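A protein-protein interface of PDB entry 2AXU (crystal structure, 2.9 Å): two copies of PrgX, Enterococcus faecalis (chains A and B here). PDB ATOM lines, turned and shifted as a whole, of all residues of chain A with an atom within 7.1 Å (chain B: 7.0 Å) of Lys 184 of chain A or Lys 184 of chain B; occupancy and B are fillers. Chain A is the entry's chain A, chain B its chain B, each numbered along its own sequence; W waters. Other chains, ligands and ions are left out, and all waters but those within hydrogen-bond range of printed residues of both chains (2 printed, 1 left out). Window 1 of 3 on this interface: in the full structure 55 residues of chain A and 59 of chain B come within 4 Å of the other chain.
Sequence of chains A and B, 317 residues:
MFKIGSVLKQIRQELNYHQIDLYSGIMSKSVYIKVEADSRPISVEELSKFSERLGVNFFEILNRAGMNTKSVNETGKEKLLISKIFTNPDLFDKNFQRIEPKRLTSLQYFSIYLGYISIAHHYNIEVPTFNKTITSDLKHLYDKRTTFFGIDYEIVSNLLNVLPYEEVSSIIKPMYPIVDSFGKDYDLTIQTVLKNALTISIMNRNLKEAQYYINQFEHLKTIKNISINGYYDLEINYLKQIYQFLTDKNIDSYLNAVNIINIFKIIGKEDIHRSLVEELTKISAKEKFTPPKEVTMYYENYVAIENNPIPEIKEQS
The backbone carbonyl oxygen (O) of Phe 182 of chain A is in hydrogen-bond range of the side-chain amide nitrogen (ND2) of Asn 63 of chain B, at 3.2 Å. OD2 of Asp 185 of chain B lies within salt-bridge range of NZ of Lys 184 of chain A (3.0 Å). O of Phe 182 of chain B sits at hydrogen-bond distance from ND2 of Asn 63 of chain A (3.3 Å). The side-chain carboxylate of Asp 185 of chain A is in salt-bridge range of the side-chain amino group of Lys 184 of chain B.
The side-chain hydroxyl (OG1) of Thr 189 of chain A lies within hydrogen-bond range of the backbone carbonyl oxygen (O) of Asp 185 of chain A. The backbone NH (N) of Gly 183 of chain A is in hydrogen-bond range of the side-chain hydroxyl (OG) of Ser 181 of chain A (3.3 Å). O of Asp 185 of chain B is in hydrogen-bond range of OG1 of Thr 189 of chain B, 3.2 Å away.
Among the printed residues, merely in contact across the chains: Asn 63 of chain A with Gly 183 of chain B (3.7 Å), Gly 183 of chain A with Asn 63 of chain B (3.98 Å) and Lys 184 of chain A with Lys 184 of chain B (3.4 Å).
Lys 184 of chain A touches just these residues of chain B: Lys 184 and Asp 185. Lys 184 of chain B touches two residues of chain A. Of the printed residues of chain B, Asn 63 of chain A touches Phe 182 (3.3 Å) and Gly 183 (3.7 Å). Of the printed residues of chain A, Phe 182 of chain B touches Asn 63. Thr 189 of chain B touches none of the printed residues of chain A. Asn 225 of chain A touches none of the printed residues of chain B. The nearest residue of chain B that does not touch Lys 184 of chain A is Leu 188 of chain B (4.2 Å). The nearest residue of chain A that does not touch Lys 184 of chain B is Leu 188 of chain A (4.5 Å).
Of the 13 printed residues of chain B, 5 touch a printed residue of chain A. Printed residues of chain A that touch a printed residue of chain B: Asn 63, Phe 182, Gly 183, Lys 184 and Asp 185. Among the printed residues, 7 pairs touch across the chains.
Asn 63 of chain A touches Phe 182 of chain B, and with the chains exchanged Phe 182 of chain A touches Asn 63 of chain B. Asn 63 of chain A touches Gly 183 of chain B, and with the chains exchanged Gly 183 of chain A touches Asn 63 of chain B. Lys 184 of chain A touches its own counterpart, Lys 184 of chain B. Lys 184 of chain A touches Asp 185 of chain B, and with the chains exchanged Asp 185 of chain A touches Lys 184 of chain B. Of the 7 pairs that touch across the chains among the printed residues, 7 have their exchanged pair printed and touching as well.
Water W2 bridges the side-chain carboxylate (OD2) of Asp 185 of chain B (2.7 Å) and the backbone NH (N) of Lys 184 of chain A (3.3 Å). Water W1 bridges the backbone NH (N) of Lys 184 of chain B (3.3 Å) and the side-chain carboxylate (OD2) of Asp 185 of chain A (3.4 Å).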
ATOM      1  N   ASN A  63      12.862 -25.332  19.545  1.00  0.00           N
ATOM      2  CA  ASN A  63      13.988 -24.501  19.945  1.00  0.00           C
ATOM      3  C   ASN A  63      13.553 -23.499  21.004  1.00  0.00           C
ATOM      4  O   ASN A  63      14.236 -23.297  21.998  1.00  0.00           O
ATOM      5  CB  ASN A  63      14.567 -23.762  18.736  1.00  0.00           C
ATOM      6  CG  ASN A  63      15.726 -24.499  18.115  1.00  0.00           C
ATOM      7  OD1 ASN A  63      16.769 -24.675  18.746  1.00  0.00           O
ATOM      8  ND2 ASN A  63      15.557 -24.937  16.874  1.00  0.00           N
ATOM      9  N   SER A 181      21.592 -34.686   2.489  1.00  0.00           N
ATOM     10  CA  SER A 181      21.607 -33.724   3.583  1.00  0.00           C
ATOM     11  C   SER A 181      20.617 -34.167   4.645  1.00  0.00           C
ATOM     12  O   SER A 181      19.616 -34.806   4.341  1.00  0.00           O
ATOM     13  CB  SER A 181      21.197 -32.337   3.086  1.00  0.00           C
ATOM     14  OG  SER A 181      20.816 -31.513   4.176  1.00  0.00           O
ATOM     15  N   PHE A 182      20.892 -33.824   5.894  1.00  0.00           N
ATOM     16  CA  PHE A 182      19.992 -34.183   6.977  1.00  0.00           C
ATOM     17  C   PHE A 182      19.814 -33.010   7.918  1.00  0.00           C
ATOM     18  O   PHE A 182      19.595 -33.185   9.118  1.00  0.00           O
ATOM     19  CB  PHE A 182      20.517 -35.417   7.713  1.00  0.00           C
ATOM     20  CG  PHE A 182      20.317 -36.689   6.944  1.00  0.00           C
ATOM     21  CD1 PHE A 182      19.048 -37.253   6.835  1.00  0.00           C
ATOM     22  CD2 PHE A 182      21.376 -37.290   6.271  1.00  0.00           C
ATOM     23  CE1 PHE A 182      18.836 -38.390   6.060  1.00  0.00           C
ATOM     24  CE2 PHE A 182      21.171 -38.429   5.490  1.00  0.00           C
ATOM     25  CZ  PHE A 182      19.899 -38.978   5.385  1.00  0.00           C
ATOM     26  N   GLY A 183      19.910 -31.806   7.357  1.00  0.00           N
ATOM     27  CA  GLY A 183      19.747 -30.608   8.157  1.00  0.00           C
ATOM     28  C   GLY A 183      20.993 -29.752   8.290  1.00  0.00           C
ATOM     29  O   GLY A 183      22.122 -30.246   8.200  1.00  0.00           O
ATOM     30  N   LYS A 184      20.779 -28.460   8.516  1.00  0.00           N
ATOM     31  CA  LYS A 184      21.873 -27.514   8.673  1.00  0.00           C
ATOM     32  C   LYS A 184      22.896 -27.964   9.724  1.00  0.00           C
ATOM     33  O   LYS A 184      24.092 -27.710   9.576  1.00  0.00           O
ATOM     34  CB  LYS A 184      21.319 -26.134   9.034  1.00  0.00           C
ATOM     35  CG  LYS A 184      20.470 -25.492   7.941  1.00  0.00           C
ATOM     36  CD  LYS A 184      20.285 -24.002   8.203  1.00  0.00           C
ATOM     37  CE  LYS A 184      19.581 -23.291   7.051  1.00  0.00           C
ATOM     38  NZ  LYS A 184      18.127 -23.608   6.972  1.00  0.00           N
ATOM     39  N   ASP A 185      22.432 -28.623  10.782  1.00  0.00           N
ATOM     40  CA  ASP A 185      23.334 -29.106  11.822  1.00  0.00           C
ATOM     41  C   ASP A 185      24.268 -30.155  11.225  1.00  0.00           C
ATOM     42  O   ASP A 185      25.487 -30.089  11.393  1.00  0.00           O
ATOM     43  CB  ASP A 185      22.548 -29.730  12.979  1.00  0.00           C
ATOM     44  CG  ASP A 185      21.757 -28.710  13.767  1.00  0.00           C
ATOM     45  OD1 ASP A 185      20.977 -29.118  14.655  1.00  0.00           O
ATOM     46  OD2 ASP A 185      21.920 -27.499  13.507  1.00  0.00           O
ATOM     47  N   TYR A 186      23.680 -31.118  10.521  1.00  0.00           N
ATOM     48  CA  TYR A 186      24.425 -32.204   9.888  1.00  0.00           C
ATOM     49  C   TYR A 186      25.360 -31.700   8.777  1.00  0.00           C
ATOM     50  O   TYR A 186      26.506 -32.146   8.678  1.00  0.00           O
ATOM     51  CB  TYR A 186      23.422 -33.225   9.344  1.00  0.00           C
ATOM     52  CG  TYR A 186      23.998 -34.353   8.520  1.00  0.00           C
ATOM     53  CD1 TYR A 186      24.259 -34.186   7.158  1.00  0.00           C
ATOM     54  CD2 TYR A 186      24.258 -35.596   9.093  1.00  0.00           C
ATOM     55  CE1 TYR A 186      24.759 -35.229   6.387  1.00  0.00           C
ATOM     56  CE2 TYR A 186      24.756 -36.648   8.331  1.00  0.00           C
ATOM     57  CZ  TYR A 186      25.005 -36.457   6.975  1.00  0.00           C
ATOM     58  OH  TYR A 186      25.494 -37.494   6.205  1.00  0.00           O
ATOM     59  N   ASP A 187      24.871 -30.775   7.952  1.00  0.00           N
ATOM     60  CA  ASP A 187      25.668 -30.208   6.866  1.00  0.00           C
ATOM     61  C   ASP A 187      26.956 -29.598   7.410  1.00  0.00           C
ATOM     62  O   ASP A 187      28.047 -29.835   6.892  1.00  0.00           O
ATOM     63  CB  ASP A 187      24.902 -29.099   6.148  1.00  0.00           C
ATOM     64  CG  ASP A 187      23.564 -29.558   5.597  1.00  0.00           C
ATOM     65  OD1 ASP A 187      22.816 -28.684   5.100  1.00  0.00           O
ATOM     66  OD2 ASP A 187      23.254 -30.771   5.657  1.00  0.00           O
ATOM     67  N   LEU A 188      26.815 -28.802   8.462  1.00  0.00           N
ATOM     68  CA  LEU A 188      27.954 -28.130   9.055  1.00  0.00           C
ATOM     69  C   LEU A 188      29.025 -29.096   9.516  1.00  0.00           C
ATOM     70  O   LEU A 188      30.209 -28.835   9.333  1.00  0.00           O
ATOM     71  CB  LEU A 188      27.488 -27.259  10.225  1.00  0.00           C
ATOM     72  CG  LEU A 188      28.442 -26.174  10.743  1.00  0.00           C
ATOM     73  CD1 LEU A 188      29.321 -26.727  11.829  1.00  0.00           C
ATOM     74  CD2 LEU A 188      29.282 -25.641   9.602  1.00  0.00           C
ATOM     75  N   THR A 189      28.620 -30.217  10.103  1.00  0.00           N
ATOM     76  CA  THR A 189      29.589 -31.192  10.595  1.00  0.00           C
ATOM     77  C   THR A 189      30.331 -31.930   9.480  1.00  0.00           C
ATOM     78  O   THR A 189      31.554 -32.072   9.538  1.00  0.00           O
ATOM     79  CB  THR A 189      28.924 -32.231  11.497  1.00  0.00           C
ATOM     80  OG1 THR A 189      27.962 -31.585  12.333  1.00  0.00           O
ATOM     81  CG2 THR A 189      29.962 -32.895  12.392  1.00  0.00           C
ATOM     82  N   GLN A 191      31.019 -30.887   6.823  1.00  0.00           N
ATOM     83  CA  GLN A 191      31.864 -29.882   6.181  1.00  0.00           C
ATOM     84  C   GLN A 191      33.126 -29.578   6.979  1.00  0.00           C
ATOM     85  O   GLN A 191      34.208 -29.416   6.410  1.00  0.00           O
ATOM     86  CB  GLN A 191      31.082 -28.585   5.992  1.00  0.00           C
ATOM     87  CG  GLN A 191      30.511 -28.398   4.608  1.00  0.00           C
ATOM     88  CD  GLN A 191      29.414 -27.354   4.582  1.00  0.00           C
ATOM     89  OE1 GLN A 191      28.302 -27.598   5.048  1.00  0.00           O
ATOM     90  NE2 GLN A 191      29.722 -26.181   4.047  1.00  0.00           N
ATOM     91  N   ASN A 225      19.537 -29.365  -1.289  1.00  0.00           N
ATOM     92  CA  ASN A 225      19.287 -28.702  -0.017  1.00  0.00           C
ATOM     93  C   ASN A 225      20.465 -28.662   0.947  1.00  0.00           C
ATOM     94  O   ASN A 225      20.295 -28.389   2.133  1.00  0.00           O
ATOM     95  CB  ASN A 225      18.077 -29.335   0.669  1.00  0.00           C
ATOM     96  CG  ASN A 225      16.819 -29.233  -0.172  1.00  0.00           C
ATOM     97  OD1 ASN A 225      16.294 -28.142  -0.401  1.00  0.00           O
ATOM     98  ND2 ASN A 225      16.335 -30.373  -0.645  1.00  0.00           N
ATOM     99  N   SER A 227      23.495 -27.074   2.773  1.00  0.00           N
ATOM    100  CA  SER A 227      23.758 -25.684   3.114  1.00  0.00           C
ATOM    101  C   SER A 227      25.256 -25.501   3.322  1.00  0.00           C
ATOM    102  O   SER A 227      25.789 -25.749   4.403  1.00  0.00           O
ATOM    103  CB  SER A 227      22.984 -25.271   4.368  1.00  0.00           C
ATOM    104  OG  SER A 227      21.801 -24.573   4.011  1.00  0.00           O
ATOM    105  N   ASN B  63      14.709 -35.543  10.741  1.00  0.00           N
ATOM    106  CA  ASN B  63      14.919 -35.392   9.308  1.00  0.00           C
ATOM    107  C   ASN B  63      15.088 -36.757   8.664  1.00  0.00           C
ATOM    108  O   ASN B  63      14.593 -36.990   7.560  1.00  0.00           O
ATOM    109  CB  ASN B  63      16.131 -34.502   9.014  1.00  0.00           C
ATOM    110  CG  ASN B  63      15.799 -33.026   9.125  1.00  0.00           C
ATOM    111  OD1 ASN B  63      14.836 -32.552   8.521  1.00  0.00           O
ATOM    112  ND2 ASN B  63      16.591 -32.292   9.897  1.00  0.00           N
ATOM    113  N   SER B 181      18.919 -16.562  19.521  1.00  0.00           N
ATOM    114  CA  SER B 181      18.947 -17.384  18.321  1.00  0.00           C
ATOM    115  C   SER B 181      17.980 -18.516  18.621  1.00  0.00           C
ATOM    116  O   SER B 181      17.867 -18.938  19.769  1.00  0.00           O
ATOM    117  CB  SER B 181      20.346 -17.959  18.098  1.00  0.00           C
ATOM    118  OG  SER B 181      20.285 -19.180  17.382  1.00  0.00           O
ATOM    119  N   PHE B 182      17.280 -19.007  17.606  1.00  0.00           N
ATOM    120  CA  PHE B 182      16.340 -20.099  17.812  1.00  0.00           C
ATOM    121  C   PHE B 182      16.538 -21.196  16.784  1.00  0.00           C
ATOM    122  O   PHE B 182      15.585 -21.733  16.222  1.00  0.00           O
ATOM    123  CB  PHE B 182      14.897 -19.578  17.792  1.00  0.00           C
ATOM    124  CG  PHE B 182      14.547 -18.767  18.998  1.00  0.00           C
ATOM    125  CD1 PHE B 182      14.456 -19.371  20.252  1.00  0.00           C
ATOM    126  CD2 PHE B 182      14.393 -17.389  18.910  1.00  0.00           C
ATOM    127  CE1 PHE B 182      14.226 -18.608  21.402  1.00  0.00           C
ATOM    128  CE2 PHE B 182      14.161 -16.619  20.057  1.00  0.00           C
ATOM    129  CZ  PHE B 182      14.080 -17.228  21.298  1.00  0.00           C
ATOM    130  N   GLY B 183      17.802 -21.529  16.555  1.00  0.00           N
ATOM    131  CA  GLY B 183      18.135 -22.570  15.604  1.00  0.00           C
ATOM    132  C   GLY B 183      18.646 -22.012  14.289  1.00  0.00           C
ATOM    133  O   GLY B 183      18.404 -20.850  13.956  1.00  0.00           O
ATOM    134  N   LYS B 184      19.344 -22.851  13.533  1.00  0.00           N
ATOM    135  CA  LYS B 184      19.894 -22.447  12.251  1.00  0.00           C
ATOM    136  C   LYS B 184      18.839 -21.983  11.248  1.00  0.00           C
ATOM    137  O   LYS B 184      19.056 -20.998  10.539  1.00  0.00           O
ATOM    138  CB  LYS B 184      20.738 -23.584  11.662  1.00  0.00           C
ATOM    139  CG  LYS B 184      22.010 -23.853  12.457  1.00  0.00           C
ATOM    140  CD  LYS B 184      22.976 -24.755  11.707  1.00  0.00           C
ATOM    141  CE  LYS B 184      24.309 -24.882  12.436  1.00  0.00           C
ATOM    142  NZ  LYS B 184      24.198 -25.655  13.708  1.00  0.00           N
ATOM    143  N   ASP B 185      17.702 -22.674  11.188  1.00  0.00           N
ATOM    144  CA  ASP B 185      16.631 -22.290  10.261  1.00  0.00           C
ATOM    145  C   ASP B 185      16.224 -20.836  10.497  1.00  0.00           C
ATOM    146  O   ASP B 185      16.130 -20.030   9.568  1.00  0.00           O
ATOM    147  CB  ASP B 185      15.406 -23.190  10.451  1.00  0.00           C
ATOM    148  CG  ASP B 185      15.629 -24.599   9.936  1.00  0.00           C
ATOM    149  OD1 ASP B 185      14.743 -25.458  10.150  1.00  0.00           O
ATOM    150  OD2 ASP B 185      16.681 -24.847   9.313  1.00  0.00           O
ATOM    151  N   TYR B 186      15.991 -20.517  11.763  1.00  0.00           N
ATOM    152  CA  TYR B 186      15.589 -19.184  12.198  1.00  0.00           C
ATOM    153  C   TYR B 186      16.679 -18.134  11.958  1.00  0.00           C
ATOM    154  O   TYR B 186      16.391 -17.036  11.474  1.00  0.00           O
ATOM    155  CB  TYR B 186      15.206 -19.262  13.684  1.00  0.00           C
ATOM    156  CG  TYR B 186      14.937 -17.953  14.373  1.00  0.00           C
ATOM    157  CD1 TYR B 186      15.974 -17.217  14.941  1.00  0.00           C
ATOM    158  CD2 TYR B 186      13.637 -17.456  14.478  1.00  0.00           C
ATOM    159  CE1 TYR B 186      15.724 -16.017  15.599  1.00  0.00           C
ATOM    160  CE2 TYR B 186      13.377 -16.259  15.132  1.00  0.00           C
ATOM    161  CZ  TYR B 186      14.423 -15.545  15.691  1.00  0.00           C
ATOM    162  OH  TYR B 186      14.170 -14.362  16.348  1.00  0.00           O
ATOM    163  N   ASP B 187      17.924 -18.483  12.288  1.00  0.00           N
ATOM    164  CA  ASP B 187      19.075 -17.588  12.133  1.00  0.00           C
ATOM    165  C   ASP B 187      19.279 -17.101  10.703  1.00  0.00           C
ATOM    166  O   ASP B 187      19.720 -15.977  10.479  1.00  0.00           O
ATOM    167  CB  ASP B 187      20.361 -18.283  12.594  1.00  0.00           C
ATOM    168  CG  ASP B 187      20.424 -18.480  14.098  1.00  0.00           C
ATOM    169  OD1 ASP B 187      21.398 -19.108  14.564  1.00  0.00           O
ATOM    170  OD2 ASP B 187      19.510 -18.013  14.813  1.00  0.00           O
ATOM    171  N   LEU B 188      18.973 -17.957   9.736  1.00  0.00           N
ATOM    172  CA  LEU B 188      19.127 -17.614   8.329  1.00  0.00           C
ATOM    173  C   LEU B 188      18.067 -16.594   7.939  1.00  0.00           C
ATOM    174  O   LEU B 188      18.368 -15.559   7.344  1.00  0.00           O
ATOM    175  CB  LEU B 188      18.963 -18.870   7.470  1.00  0.00           C
ATOM    176  CG  LEU B 188      19.635 -19.004   6.097  1.00  0.00           C
ATOM    177  CD1 LEU B 188      18.645 -19.659   5.146  1.00  0.00           C
ATOM    178  CD2 LEU B 188      20.071 -17.649   5.550  1.00  0.00           C
ATOM    179  N   THR B 189      16.819 -16.902   8.274  1.00  0.00           N
ATOM    180  CA  THR B 189      15.687 -16.033   7.965  1.00  0.00           C
ATOM    181  C   THR B 189      15.900 -14.596   8.415  1.00  0.00           C
ATOM    182  O   THR B 189      15.694 -13.655   7.651  1.00  0.00           O
ATOM    183  CB  THR B 189      14.403 -16.535   8.632  1.00  0.00           C
ATOM    184  OG1 THR B 189      14.137 -17.881   8.218  1.00  0.00           O
ATOM    185  CG2 THR B 189      13.233 -15.649   8.249  1.00  0.00           C
ATOM    186  N   GLN B 191      18.605 -13.047   8.920  1.00  0.00           N
ATOM    187  CA  GLN B 191      19.709 -12.405   8.212  1.00  0.00           C
ATOM    188  C   GLN B 191      19.302 -12.013   6.802  1.00  0.00           C
ATOM    189  O   GLN B 191      19.779 -11.008   6.266  1.00  0.00           O
ATOM    190  CB  GLN B 191      20.932 -13.327   8.150  1.00  0.00           C
ATOM    191  CG  GLN B 191      21.442 -13.782   9.508  1.00  0.00           C
ATOM    192  CD  GLN B 191      22.694 -14.633   9.402  1.00  0.00           C
ATOM    193  OE1 GLN B 191      22.806 -15.676  10.044  1.00  0.00           O
ATOM    194  NE2 GLN B 191      23.646 -14.189   8.591  1.00  0.00           N
ATOM    195  N   ASN B 225      25.457 -18.392  20.107  1.00  0.00           N
ATOM    196  CA  ASN B 225      25.028 -19.503  19.262  1.00  0.00           C
ATOM    197  C   ASN B 225      24.478 -19.116  17.897  1.00  0.00           C
ATOM    198  O   ASN B 225      24.120 -19.984  17.106  1.00  0.00           O
ATOM    199  CB  ASN B 225      23.995 -20.359  19.995  1.00  0.00           C
ATOM    200  CG  ASN B 225      24.494 -20.839  21.339  1.00  0.00           C
ATOM    201  OD1 ASN B 225      25.553 -21.461  21.434  1.00  0.00           O
ATOM    202  ND2 ASN B 225      23.735 -20.553  22.389  1.00  0.00           N
ATOM    203  N   SER B 227      24.257 -18.415  14.147  1.00  0.00           N
ATOM    204  CA  SER B 227      25.049 -18.981  13.053  1.00  0.00           C
ATOM    205  C   SER B 227      25.018 -17.990  11.901  1.00  0.00           C
ATOM    206  O   SER B 227      24.048 -17.949  11.149  1.00  0.00           O
ATOM    207  CB  SER B 227      24.452 -20.308  12.585  1.00  0.00           C
ATOM    208  OG  SER B 227      24.285 -21.206  13.668  1.00  0.00           O
HETATM  209  O   HOH W   1      19.313 -25.843  14.917  1.00  0.00           O
HETATM  210  O   HOH W   2      17.769 -27.354   9.182  1.00  0.00           O
